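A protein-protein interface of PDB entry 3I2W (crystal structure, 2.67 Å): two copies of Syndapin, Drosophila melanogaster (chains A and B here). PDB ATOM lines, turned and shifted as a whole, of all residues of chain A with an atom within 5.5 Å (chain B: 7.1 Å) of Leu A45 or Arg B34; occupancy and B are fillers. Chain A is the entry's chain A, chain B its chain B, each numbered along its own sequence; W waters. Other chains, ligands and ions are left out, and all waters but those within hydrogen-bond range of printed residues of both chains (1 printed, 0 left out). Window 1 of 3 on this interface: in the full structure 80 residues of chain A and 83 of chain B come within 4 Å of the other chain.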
ATOM      1  N   GLY A  40     -16.128 -17.089  19.769  1.00  0.00           N
ATOM      2  CA  GLY A  40     -16.783 -16.596  18.578  1.00  0.00           C
ATOM      3  C   GLY A  40     -16.798 -17.711  17.570  1.00  0.00           C
ATOM      4  O   GLY A  40     -17.810 -17.950  16.930  1.00  0.00           O
ATOM      5  N   TYR A  41     -15.658 -18.396  17.459  1.00  0.00           N
ATOM      6  CA  TYR A  41     -15.490 -19.522  16.600  1.00  0.00           C
ATOM      7  C   TYR A  41     -16.510 -20.581  16.949  1.00  0.00           C
ATOM      8  O   TYR A  41     -17.122 -21.142  16.101  1.00  0.00           O
ATOM      9  CB  TYR A  41     -14.084 -20.058  16.794  1.00  0.00           C
ATOM     10  CG  TYR A  41     -13.653 -21.125  15.820  1.00  0.00           C
ATOM     11  CD1 TYR A  41     -13.907 -21.016  14.483  1.00  0.00           C
ATOM     12  CD2 TYR A  41     -12.977 -22.213  16.255  1.00  0.00           C
ATOM     13  CE1 TYR A  41     -13.527 -21.979  13.641  1.00  0.00           C
ATOM     14  CE2 TYR A  41     -12.614 -23.178  15.429  1.00  0.00           C
ATOM     15  CZ  TYR A  41     -12.877 -23.076  14.130  1.00  0.00           C
ATOM     16  OH  TYR A  41     -12.416 -24.053  13.291  1.00  0.00           O
ATOM     17  N   ALA A  42     -16.710 -20.831  18.222  1.00  0.00           N
ATOM     18  CA  ALA A  42     -17.546 -21.892  18.656  1.00  0.00           C
ATOM     19  C   ALA A  42     -18.969 -21.493  18.376  1.00  0.00           C
ATOM     20  O   ALA A  42     -19.793 -22.336  18.025  1.00  0.00           O
ATOM     21  CB  ALA A  42     -17.331 -22.089  20.118  1.00  0.00           C
ATOM     22  N   LYS A  43     -19.303 -20.222  18.521  1.00  0.00           N
ATOM     23  CA  LYS A  43     -20.708 -19.910  18.346  1.00  0.00           C
ATOM     24  C   LYS A  43     -21.023 -20.081  16.864  1.00  0.00           C
ATOM     25  O   LYS A  43     -21.995 -20.712  16.510  1.00  0.00           O
ATOM     26  CB  LYS A  43     -21.085 -18.505  18.807  1.00  0.00           C
ATOM     27  CG  LYS A  43     -21.642 -18.418  20.196  1.00  0.00           C
ATOM     28  CD  LYS A  43     -22.685 -17.290  20.218  1.00  0.00           C
ATOM     29  CE  LYS A  43     -22.655 -16.434  21.524  1.00  0.00           C
ATOM     30  NZ  LYS A  43     -22.911 -17.195  22.794  1.00  0.00           N
ATOM     31  N   SER A  44     -20.180 -19.503  16.022  1.00  0.00           N
ATOM     32  CA  SER A  44     -20.222 -19.662  14.590  1.00  0.00           C
ATOM     33  C   SER A  44     -20.366 -21.096  14.095  1.00  0.00           C
ATOM     34  O   SER A  44     -21.201 -21.394  13.237  1.00  0.00           O
ATOM     35  CB  SER A  44     -18.951 -19.100  14.026  1.00  0.00           C
ATOM     36  OG  SER A  44     -19.146 -17.731  13.928  1.00  0.00           O
ATOM     37  N   LEU A  45     -19.555 -21.974  14.639  1.00  0.00           N
ATOM     38  CA  LEU A  45     -19.629 -23.314  14.254  1.00  0.00           C
ATOM     39  C   LEU A  45     -21.031 -23.842  14.477  1.00  0.00           C
ATOM     40  O   LEU A  45     -21.567 -24.485  13.607  1.00  0.00           O
ATOM     41  CB  LEU A  45     -18.567 -24.127  14.983  1.00  0.00           C
ATOM     42  CG  LEU A  45     -17.185 -23.793  14.393  1.00  0.00           C
ATOM     43  CD1 LEU A  45     -16.176 -24.415  15.170  1.00  0.00           C
ATOM     44  CD2 LEU A  45     -16.997 -24.208  12.953  1.00  0.00           C
ATOM     45  N   ARG A  46     -21.647 -23.530  15.606  1.00  0.00           N
ATOM     46  CA  ARG A  46     -22.940 -24.090  15.951  1.00  0.00           C
ATOM     47  C   ARG A  46     -24.089 -23.500  15.161  1.00  0.00           C
ATOM     48  O   ARG A  46     -25.053 -24.164  14.835  1.00  0.00           O
ATOM     49  CB  ARG A  46     -23.165 -23.898  17.426  1.00  0.00           C
ATOM     50  CG  ARG A  46     -22.231 -24.746  18.314  1.00  0.00           C
ATOM     51  CD  ARG A  46     -22.367 -24.324  19.809  1.00  0.00           C
ATOM     52  NE  ARG A  46     -21.504 -25.166  20.684  1.00  0.00           N
ATOM     53  CZ  ARG A  46     -21.294 -25.004  22.000  1.00  0.00           C
ATOM     54  NH1 ARG A  46     -21.857 -24.002  22.680  1.00  0.00           N
ATOM     55  NH2 ARG A  46     -20.509 -25.861  22.644  1.00  0.00           N
ATOM     56  N   THR A  47     -23.991 -22.240  14.826  1.00  0.00           N
ATOM     57  CA  THR A  47     -24.991 -21.602  13.999  1.00  0.00           C
ATOM     58  C   THR A  47     -24.969 -22.320  12.664  1.00  0.00           C
ATOM     59  O   THR A  47     -26.000 -22.668  12.102  1.00  0.00           O
ATOM     60  CB  THR A  47     -24.621 -20.134  13.876  1.00  0.00           C
ATOM     61  OG1 THR A  47     -24.569 -19.590  15.195  1.00  0.00           O
ATOM     62  CG2 THR A  47     -25.630 -19.343  13.076  1.00  0.00           C
ATOM     63  N   TRP A  48     -23.762 -22.599  12.195  1.00  0.00           N
ATOM     64  CA  TRP A  48     -23.571 -23.208  10.899  1.00  0.00           C
ATOM     65  C   TRP A  48     -24.093 -24.618  10.980  1.00  0.00           C
ATOM     66  O   TRP A  48     -24.779 -25.091  10.080  1.00  0.00           O
ATOM     67  CB  TRP A  48     -22.089 -23.225  10.584  1.00  0.00           C
ATOM     68  CG  TRP A  48     -21.713 -23.828   9.319  1.00  0.00           C
ATOM     69  CD1 TRP A  48     -21.744 -23.243   8.080  1.00  0.00           C
ATOM     70  CD2 TRP A  48     -21.178 -25.133   9.138  1.00  0.00           C
ATOM     71  NE1 TRP A  48     -21.273 -24.127   7.139  1.00  0.00           N
ATOM     72  CE2 TRP A  48     -20.921 -25.293   7.768  1.00  0.00           C
ATOM     73  CE3 TRP A  48     -20.899 -26.193  10.000  1.00  0.00           C
ATOM     74  CZ2 TRP A  48     -20.398 -26.463   7.253  1.00  0.00           C
ATOM     75  CZ3 TRP A  48     -20.366 -27.380   9.473  1.00  0.00           C
ATOM     76  CH2 TRP A  48     -20.125 -27.501   8.137  1.00  0.00           C
ATOM     77  N   SER A  49     -23.781 -25.292  12.064  1.00  0.00           N
ATOM     78  CA  SER A  49     -24.225 -26.603  12.201  1.00  0.00           C
ATOM     79  C   SER A  49     -25.769 -26.686  12.202  1.00  0.00           C
ATOM     80  O   SER A  49     -26.353 -27.592  11.634  1.00  0.00           O
ATOM     81  CB  SER A  49     -23.678 -27.145  13.490  1.00  0.00           C
ATOM     82  OG  SER A  49     -23.974 -28.517  13.532  1.00  0.00           O
ATOM     83  N   LYS A  50     -26.436 -25.745  12.842  1.00  0.00           N
ATOM     84  CA  LYS A  50     -27.867 -25.838  13.014  1.00  0.00           C
ATOM     85  C   LYS A  50     -28.544 -25.556  11.700  1.00  0.00           C
ATOM     86  O   LYS A  50     -29.492 -26.243  11.337  1.00  0.00           O
ATOM     87  CB  LYS A  50     -28.328 -24.853  14.101  1.00  0.00           C
ATOM     88  CG  LYS A  50     -29.825 -24.783  14.331  1.00  0.00           C
ATOM     89  CD  LYS A  50     -30.167 -24.138  15.674  1.00  0.00           C
ATOM     90  CE  LYS A  50     -31.711 -24.022  15.849  1.00  0.00           C
ATOM     91  NZ  LYS A  50     -32.386 -23.444  14.603  1.00  0.00           N
ATOM     92  N   VAL A  72     -19.861 -33.869   9.030  1.00  0.00           N
ATOM     93  CA  VAL A  72     -19.356 -32.504   9.183  1.00  0.00           C
ATOM     94  C   VAL A  72     -20.088 -31.778  10.293  1.00  0.00           C
ATOM     95  O   VAL A  72     -19.480 -31.223  11.157  1.00  0.00           O
ATOM     96  CB  VAL A  72     -19.591 -31.642   7.937  1.00  0.00           C
ATOM     97  CG1 VAL A  72     -18.967 -30.395   8.149  1.00  0.00           C
ATOM     98  CG2 VAL A  72     -18.857 -32.149   6.815  1.00  0.00           C
ATOM     99  N   GLU A  75     -18.738 -32.899  13.518  1.00  0.00           N
ATOM    100  CA  GLU A  75     -17.366 -32.602  13.857  1.00  0.00           C
ATOM    101  C   GLU A  75     -17.358 -31.150  14.290  1.00  0.00           C
ATOM    102  O   GLU A  75     -16.556 -30.711  15.148  1.00  0.00           O
ATOM    103  CB  GLU A  75     -16.435 -32.830  12.661  1.00  0.00           C
ATOM    104  CG  GLU A  75     -16.524 -31.750  11.714  1.00  0.00           C
ATOM    105  CD  GLU A  75     -15.388 -30.736  11.808  1.00  0.00           C
ATOM    106  OE1 GLU A  75     -14.206 -31.137  12.039  1.00  0.00           O
ATOM    107  OE2 GLU A  75     -15.697 -29.530  11.596  1.00  0.00           O
ATOM    108  N   SER A  76     -18.261 -30.394  13.684  1.00  0.00           N
ATOM    109  CA  SER A  76     -18.186 -28.985  13.846  1.00  0.00           C
ATOM    110  C   SER A  76     -18.627 -28.790  15.251  1.00  0.00           C
ATOM    111  O   SER A  76     -18.116 -27.949  15.950  1.00  0.00           O
ATOM    112  CB  SER A  76     -19.109 -28.276  12.883  1.00  0.00           C
ATOM    113  OG  SER A  76     -20.413 -28.445  13.343  1.00  0.00           O
ATOM    114  N   ILE A  79     -15.758 -29.542  17.644  1.00  0.00           N
ATOM    115  CA  ILE A  79     -14.739 -28.538  17.662  1.00  0.00           C
ATOM    116  C   ILE A  79     -15.252 -27.361  18.497  1.00  0.00           C
ATOM    117  O   ILE A  79     -14.535 -26.843  19.398  1.00  0.00           O
ATOM    118  CB  ILE A  79     -14.327 -28.116  16.212  1.00  0.00           C
ATOM    119  CG1 ILE A  79     -13.162 -28.946  15.688  1.00  0.00           C
ATOM    120  CG2 ILE A  79     -13.729 -26.733  16.153  1.00  0.00           C
ATOM    121  CD1 ILE A  79     -12.882 -30.143  16.459  1.00  0.00           C
ATOM    122  N   SER A  80     -16.477 -26.929  18.260  1.00  0.00           N
ATOM    123  CA  SER A  80     -16.979 -25.867  19.091  1.00  0.00           C
ATOM    124  C   SER A  80     -16.815 -26.187  20.586  1.00  0.00           C
ATOM    125  O   SER A  80     -16.574 -25.320  21.390  1.00  0.00           O
ATOM    126  CB  SER A  80     -18.449 -25.674  18.845  1.00  0.00           C
ATOM    127  OG  SER A  80     -19.132 -26.742  19.492  1.00  0.00           O
ATOM    128  N   HIS A  83     -13.333 -25.385  21.838  1.00  0.00           N
ATOM    129  CA  HIS A  83     -12.994 -24.019  21.986  1.00  0.00           C
ATOM    130  C   HIS A  83     -13.768 -23.443  23.140  1.00  0.00           C
ATOM    131  O   HIS A  83     -13.356 -22.450  23.743  1.00  0.00           O
ATOM    132  CB  HIS A  83     -13.223 -23.279  20.680  1.00  0.00           C
ATOM    133  CG  HIS A  83     -12.145 -23.559  19.678  1.00  0.00           C
ATOM    134  ND1 HIS A  83     -12.172 -24.647  18.831  1.00  0.00           N
ATOM    135  CD2 HIS A  83     -10.961 -22.953  19.463  1.00  0.00           C
ATOM    136  CE1 HIS A  83     -11.060 -24.681  18.126  1.00  0.00           C
ATOM    137  NE2 HIS A  83     -10.317 -23.658  18.488  1.00  0.00           N
ATOM    138  N   TYR A 252     -11.973 -36.964  14.766  1.00  0.00           N
ATOM    139  CA  TYR A 252     -11.771 -37.158  13.354  1.00  0.00           C
ATOM    140  C   TYR A 252     -11.851 -38.596  12.904  1.00  0.00           C
ATOM    141  O   TYR A 252     -11.995 -38.849  11.720  1.00  0.00           O
ATOM    142  CB  TYR A 252     -10.521 -36.437  12.854  1.00  0.00           C
ATOM    143  CG  TYR A 252     -10.775 -34.985  12.878  1.00  0.00           C
ATOM    144  CD1 TYR A 252     -11.526 -34.390  11.901  1.00  0.00           C
ATOM    145  CD2 TYR A 252     -10.324 -34.205  13.913  1.00  0.00           C
ATOM    146  CE1 TYR A 252     -11.796 -33.023  11.939  1.00  0.00           C
ATOM    147  CE2 TYR A 252     -10.586 -32.852  13.950  1.00  0.00           C
ATOM    148  CZ  TYR A 252     -11.326 -32.277  12.970  1.00  0.00           C
ATOM    149  OH  TYR A 252     -11.611 -30.942  13.029  1.00  0.00           O
ATOM    150  N   GLN B  28     -21.456 -27.069  -2.256  1.00  0.00           N
ATOM    151  CA  GLN B  28     -20.482 -26.021  -2.484  1.00  0.00           C
ATOM    152  C   GLN B  28     -20.786 -24.958  -1.491  1.00  0.00           C
ATOM    153  O   GLN B  28     -19.898 -24.480  -0.813  1.00  0.00           O
ATOM    154  CB  GLN B  28     -20.505 -25.481  -3.908  1.00  0.00           C
ATOM    155  CG  GLN B  28     -19.786 -26.310  -4.930  1.00  0.00           C
ATOM    156  CD  GLN B  28     -20.163 -25.889  -6.371  1.00  0.00           C
ATOM    157  OE1 GLN B  28     -19.504 -25.026  -7.011  1.00  0.00           O
ATOM    158  NE2 GLN B  28     -21.247 -26.482  -6.880  1.00  0.00           N
ATOM    159  N   GLN B  29     -22.055 -24.620  -1.358  1.00  0.00           N
ATOM    160  CA  GLN B  29     -22.443 -23.581  -0.447  1.00  0.00           C
ATOM    161  C   GLN B  29     -22.109 -23.907   0.993  1.00  0.00           C
ATOM    162  O   GLN B  29     -21.680 -23.056   1.727  1.00  0.00           O
ATOM    163  CB  GLN B  29     -23.897 -23.276  -0.576  1.00  0.00           C
ATOM    164  CG  GLN B  29     -24.328 -22.282   0.433  1.00  0.00           C
ATOM    165  CD  GLN B  29     -25.796 -21.937   0.302  1.00  0.00           C
ATOM    166  OE1 GLN B  29     -26.374 -22.004  -0.812  1.00  0.00           O
ATOM    167  NE2 GLN B  29     -26.412 -21.541   1.430  1.00  0.00           N
ATOM    168  N   LEU B  30     -22.282 -25.140   1.408  1.00  0.00           N
ATOM    169  CA  LEU B  30     -21.999 -25.516   2.772  1.00  0.00           C
ATOM    170  C   LEU B  30     -20.499 -25.374   2.993  1.00  0.00           C
ATOM    171  O   LEU B  30     -20.073 -24.822   3.998  1.00  0.00           O
ATOM    172  CB  LEU B  30     -22.509 -26.943   3.030  1.00  0.00           C
ATOM    173  CG  LEU B  30     -22.246 -27.724   4.316  1.00  0.00           C
ATOM    174  CD1 LEU B  30     -23.173 -28.914   4.555  1.00  0.00           C
ATOM    175  CD2 LEU B  30     -20.837 -28.248   4.356  1.00  0.00           C
ATOM    176  N   ILE B  31     -19.672 -25.835   2.076  1.00  0.00           N
ATOM    177  CA  ILE B  31     -18.249 -25.795   2.315  1.00  0.00           C
ATOM    178  C   ILE B  31     -17.790 -24.353   2.352  1.00  0.00           C
ATOM    179  O   ILE B  31     -17.049 -23.960   3.240  1.00  0.00           O
ATOM    180  CB  ILE B  31     -17.534 -26.615   1.220  1.00  0.00           C
ATOM    181  CG1 ILE B  31     -17.718 -28.083   1.535  1.00  0.00           C
ATOM    182  CG2 ILE B  31     -16.079 -26.239   1.056  1.00  0.00           C
ATOM    183  CD1 ILE B  31     -17.665 -28.921   0.343  1.00  0.00           C
ATOM    184  N   GLN B  32     -18.233 -23.546   1.395  1.00  0.00           N
ATOM    185  CA  GLN B  32     -17.790 -22.171   1.302  1.00  0.00           C
ATOM    186  C   GLN B  32     -18.091 -21.523   2.646  1.00  0.00           C
ATOM    187  O   GLN B  32     -17.272 -20.781   3.208  1.00  0.00           O
ATOM    188  CB  GLN B  32     -18.524 -21.459   0.186  1.00  0.00           C
ATOM    189  CG  GLN B  32     -18.264 -19.950   0.080  1.00  0.00           C
ATOM    190  CD  GLN B  32     -16.938 -19.626  -0.634  1.00  0.00           C
ATOM    191  OE1 GLN B  32     -16.740 -19.939  -1.842  1.00  0.00           O
ATOM    192  NE2 GLN B  32     -16.015 -19.010   0.102  1.00  0.00           N
ATOM    193  N   GLU B  33     -19.262 -21.859   3.182  1.00  0.00           N
ATOM    194  CA  GLU B  33     -19.686 -21.294   4.417  1.00  0.00           C
ATOM    195  C   GLU B  33     -18.764 -21.629   5.552  1.00  0.00           C
ATOM    196  O   GLU B  33     -18.410 -20.734   6.286  1.00  0.00           O
ATOM    197  CB  GLU B  33     -21.138 -21.589   4.693  1.00  0.00           C
ATOM    198  CG  GLU B  33     -21.967 -20.397   4.207  1.00  0.00           C
ATOM    199  CD  GLU B  33     -23.496 -20.560   4.164  1.00  0.00           C
ATOM    200  OE1 GLU B  33     -24.098 -21.156   5.066  1.00  0.00           O
ATOM    201  OE2 GLU B  33     -24.112 -20.024   3.210  1.00  0.00           O
ATOM    202  N   ARG B  34     -18.338 -22.877   5.693  1.00  0.00           N
ATOM    203  CA  ARG B  34     -17.401 -23.260   6.722  1.00  0.00           C
ATOM    204  C   ARG B  34     -16.104 -22.499   6.527  1.00  0.00           C
ATOM    205  O   ARG B  34     -15.479 -22.038   7.469  1.00  0.00           O
ATOM    206  CB  ARG B  34     -17.138 -24.750   6.586  1.00  0.00           C
ATOM    207  CG  ARG B  34     -16.089 -25.378   7.521  1.00  0.00           C
ATOM    208  CD  ARG B  34     -16.300 -24.997   8.964  1.00  0.00           C
ATOM    209  NE  ARG B  34     -15.377 -25.683   9.822  1.00  0.00           N
ATOM    210  CZ  ARG B  34     -15.575 -26.884  10.338  1.00  0.00           C
ATOM    211  NH1 ARG B  34     -16.685 -27.539  10.095  1.00  0.00           N
ATOM    212  NH2 ARG B  34     -14.655 -27.422  11.114  1.00  0.00           N
ATOM    213  N   ALA B  35     -15.677 -22.401   5.280  1.00  0.00           N
ATOM    214  CA  ALA B  35     -14.506 -21.606   4.904  1.00  0.00           C
ATOM    215  C   ALA B  35     -14.560 -20.200   5.405  1.00  0.00           C
ATOM    216  O   ALA B  35     -13.549 -19.615   5.665  1.00  0.00           O
ATOM    217  CB  ALA B  35     -14.382 -21.581   3.408  1.00  0.00           C
ATOM    218  N   ASP B  36     -15.735 -19.610   5.483  1.00  0.00           N
ATOM    219  CA  ASP B  36     -15.794 -18.217   5.873  1.00  0.00           C
ATOM    220  C   ASP B  36     -15.605 -18.185   7.374  1.00  0.00           C
ATOM    221  O   ASP B  36     -14.937 -17.322   7.908  1.00  0.00           O
ATOM    222  CB  ASP B  36     -17.130 -17.593   5.550  1.00  0.00           C
ATOM    223  CG  ASP B  36     -17.424 -17.545   4.089  1.00  0.00           C
ATOM    224  OD1 ASP B  36     -16.489 -17.608   3.278  1.00  0.00           O
ATOM    225  OD2 ASP B  36     -18.635 -17.417   3.738  1.00  0.00           O
ATOM    226  N   ILE B  37     -16.213 -19.132   8.054  1.00  0.00           N
ATOM    227  CA  ILE B  37     -15.988 -19.263   9.453  1.00  0.00           C
ATOM    228  C   ILE B  37     -14.495 -19.415   9.781  1.00  0.00           C
ATOM    229  O   ILE B  37     -14.018 -18.812  10.750  1.00  0.00           O
ATOM    230  CB  ILE B  37     -16.856 -20.355  10.049  1.00  0.00           C
ATOM    231  CG1 ILE B  37     -18.240 -19.780  10.226  1.00  0.00           C
ATOM    232  CG2 ILE B  37     -16.331 -20.814  11.385  1.00  0.00           C
ATOM    233  CD1 ILE B  37     -19.329 -20.804  10.203  1.00  0.00           C
ATOM    234  N   GLU B  38     -13.746 -20.153   8.979  1.00  0.00           N
ATOM    235  CA  GLU B  38     -12.347 -20.330   9.321  1.00  0.00           C
ATOM    236  C   GLU B  38     -11.592 -19.058   8.993  1.00  0.00           C
ATOM    237  O   GLU B  38     -10.789 -18.623   9.801  1.00  0.00           O
ATOM    238  CB  GLU B  38     -11.733 -21.574   8.698  1.00  0.00           C
ATOM    239  CG  GLU B  38     -12.626 -22.813   8.787  1.00  0.00           C
ATOM    240  CD  GLU B  38     -12.489 -23.521  10.100  1.00  0.00           C
ATOM    241  OE1 GLU B  38     -11.359 -23.702  10.509  1.00  0.00           O
ATOM    242  OE2 GLU B  38     -13.484 -23.914  10.734  1.00  0.00           O
ATOM    243  N   LYS B  39     -11.880 -18.448   7.843  1.00  0.00           N
ATOM    244  CA  LYS B  39     -11.347 -17.111   7.489  1.00  0.00           C
ATOM    245  C   LYS B  39     -11.619 -16.178   8.624  1.00  0.00           C
ATOM    246  O   LYS B  39     -10.748 -15.472   9.021  1.00  0.00           O
ATOM    247  CB  LYS B  39     -12.060 -16.547   6.251  1.00  0.00           C
ATOM    248  CG  LYS B  39     -11.315 -15.501   5.447  1.00  0.00           C
ATOM    249  CD  LYS B  39     -12.243 -14.690   4.471  1.00  0.00           C
ATOM    250  CE  LYS B  39     -11.407 -13.710   3.575  1.00  0.00           C
ATOM    251  NZ  LYS B  39     -10.171 -14.394   2.920  1.00  0.00           N
ATOM    252  N   GLY B  40     -12.825 -16.201   9.180  1.00  0.00           N
ATOM    253  CA  GLY B  40     -13.246 -15.227  10.165  1.00  0.00           C
ATOM    254  C   GLY B  40     -12.506 -15.370  11.483  1.00  0.00           C
ATOM    255  O   GLY B  40     -12.318 -14.390  12.180  1.00  0.00           O
ATOM    256  N   ILE B  86      -6.878 -23.917   5.766  1.00  0.00           N
ATOM    257  CA  ILE B  86      -8.059 -24.727   5.673  1.00  0.00           C
ATOM    258  C   ILE B  86      -9.070 -23.981   4.807  1.00  0.00           C
ATOM    259  O   ILE B  86      -9.685 -24.534   3.911  1.00  0.00           O
ATOM    260  CB  ILE B  86      -8.661 -24.992   7.024  1.00  0.00           C
ATOM    261  CG1 ILE B  86      -7.661 -25.707   7.903  1.00  0.00           C
ATOM    262  CG2 ILE B  86      -9.862 -25.874   6.901  1.00  0.00           C
ATOM    263  CD1 ILE B  86      -8.221 -25.993   9.240  1.00  0.00           C
ATOM    264  N   LYS B  87      -9.226 -22.700   5.033  1.00  0.00           N
ATOM    265  CA  LYS B  87     -10.062 -21.910   4.132  1.00  0.00           C
ATOM    266  C   LYS B  87      -9.644 -22.092   2.669  1.00  0.00           C
ATOM    267  O   LYS B  87     -10.470 -22.181   1.763  1.00  0.00           O
ATOM    268  CB  LYS B  87      -9.970 -20.451   4.537  1.00  0.00           C
ATOM    269  CG  LYS B  87     -10.786 -19.583   3.678  1.00  0.00           C
ATOM    270  CD  LYS B  87      -9.925 -18.690   2.840  1.00  0.00           C
ATOM    271  CE  LYS B  87     -10.726 -18.198   1.660  1.00  0.00           C
ATOM    272  NZ  LYS B  87      -9.876 -17.190   0.965  1.00  0.00           N
ATOM    273  N   LEU B  90     -10.286 -25.719   1.392  1.00  0.00           N
ATOM    274  CA  LEU B  90     -11.684 -26.025   1.154  1.00  0.00           C
ATOM    275  C   LEU B  90     -12.047 -25.369  -0.144  1.00  0.00           C
ATOM    276  O   LEU B  90     -12.682 -25.973  -0.975  1.00  0.00           O
ATOM    277  CB  LEU B  90     -12.589 -25.508   2.249  1.00  0.00           C
ATOM    278  CG  LEU B  90     -12.477 -26.110   3.638  1.00  0.00           C
ATOM    279  CD1 LEU B  90     -13.357 -25.335   4.550  1.00  0.00           C
ATOM    280  CD2 LEU B  90     -12.822 -27.558   3.726  1.00  0.00           C
ATOM    281  N   VAL B 236     -12.990 -33.280   2.255  1.00  0.00           N
ATOM    282  CA  VAL B 236     -13.317 -32.269   3.228  1.00  0.00           C
ATOM    283  C   VAL B 236     -12.627 -32.645   4.521  1.00  0.00           C
ATOM    284  O   VAL B 236     -11.823 -31.848   5.083  1.00  0.00           O
ATOM    285  CB  VAL B 236     -14.808 -32.205   3.516  1.00  0.00           C
ATOM    286  CG1 VAL B 236     -15.053 -31.212   4.591  1.00  0.00           C
ATOM    287  CG2 VAL B 236     -15.559 -31.740   2.325  1.00  0.00           C
ATOM    288  N   LEU B 240      -9.895 -30.623   7.182  1.00  0.00           N
ATOM    289  CA  LEU B 240     -10.227 -30.175   8.500  1.00  0.00           C
ATOM    290  C   LEU B 240      -9.470 -30.916   9.587  1.00  0.00           C
ATOM    291  O   LEU B 240      -9.468 -30.497  10.716  1.00  0.00           O
ATOM    292  CB  LEU B 240     -11.725 -30.344   8.760  1.00  0.00           C
ATOM    293  CG  LEU B 240     -12.726 -29.295   8.320  1.00  0.00           C
ATOM    294  CD1 LEU B 240     -12.407 -29.027   6.990  1.00  0.00           C
ATOM    295  CD2 LEU B 240     -14.085 -29.932   8.312  1.00  0.00           C
HETATM  296  O   HOH W   1     -11.226 -28.773  11.930  1.00  0.00           O
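Of the printed residues of chain B, Ser A44 touches Ile B37. Leu A45 touches two residues of chain B. Of the printed residues of chain B, Tyr A252 touches Leu B240. Gln B32 touches none of the printed residues of chain A. Arg B34 touches just these residues of chain A: Leu A45, Trp A48, Glu A75 and Ser A76. Val B236 touches none of the printed residues of chain A. The nearest residue of chain B that does not touch Leu A45 is Glu B38 (4.2 Å). The nearest printed residue of chain B that does not touch Glu A75 is Glu B38 (6.1 Å).
The side-chain carboxylate (OE1) of Glu A75 is in hydrogen-bond range of the side-chain hydroxyl (OH) of Tyr A252 (2.8 Å). NE2 of Gln B29 sits at hydrogen-bond distance from OE2 of Glu B33. The side-chain hydroxyl of Ser A44 is in hydrogen-bond range of the backbone carbonyl oxygen of Gly A40 (3.3 Å). NE of Arg B34 is in salt-bridge range of OE2 of Glu B38, at 2.7 Å.
Of the 18 printed residues of chain A, 7 touch a printed residue of chain B. Of the 18 printed residues of chain B, 6 touch a printed residue of chain A. Printed residues of chain B that touch a printed residue of chain A: Leu B30, Glu B33, Arg B34, Ile B37, Glu B38 and Leu B240. Among the printed residues, 13 pairs touch across the chains. Among the printed residues, Asp or Glu carboxylates within 4 Å of a Lys or Arg side-chain nitrogen of the other chain: Glu A75 with Arg B34 (2.4 Å).
Water W1 lies within hydrogen-bond range of OH of Tyr A252 and O of Leu B240.
Among the printed residues, merely in contact across the chains: Tyr A41 with Ile B37 (3.8 Å), Ser A44 with Ile B37 (3.6 Å), Leu A45 with Arg B34 (3.8 Å), Leu A45 with Ile B37 (3.8 Å), Trp A48 with Glu B33 (3.5 Å), Trp A48 with Arg B34 (3.5 Å), Trp A48 with Ile B37 (3.7 Å), Glu A75 with Leu B240 (3.7 Å) and Ser A76 with Arg B34 (3.8 Å).
1 position is printed for both chains. Of the 13 pairs that touch across the chains among the printed residues, none has its exchanged pair printed and touching as well.
The side-chain carboxylate (OE2) of Glu A75 is in salt-bridge range of the guanidinium group (NH2) of Arg B34 (2.4 Å). The side-chain hydroxyl (OH) of Tyr A41 sits at hydrogen-bond distance from the side-chain carboxylate (OE2) of Glu B38, at 2.8 Å. The backbone carbonyl oxygen (O) of Leu B240 sits at hydrogen-bond distance from the side-chain hydroxyl (OH) of Tyr A252. NE1 of Trp A48 lies within hydrogen-bond range of O of Leu B30 (3.4 Å).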
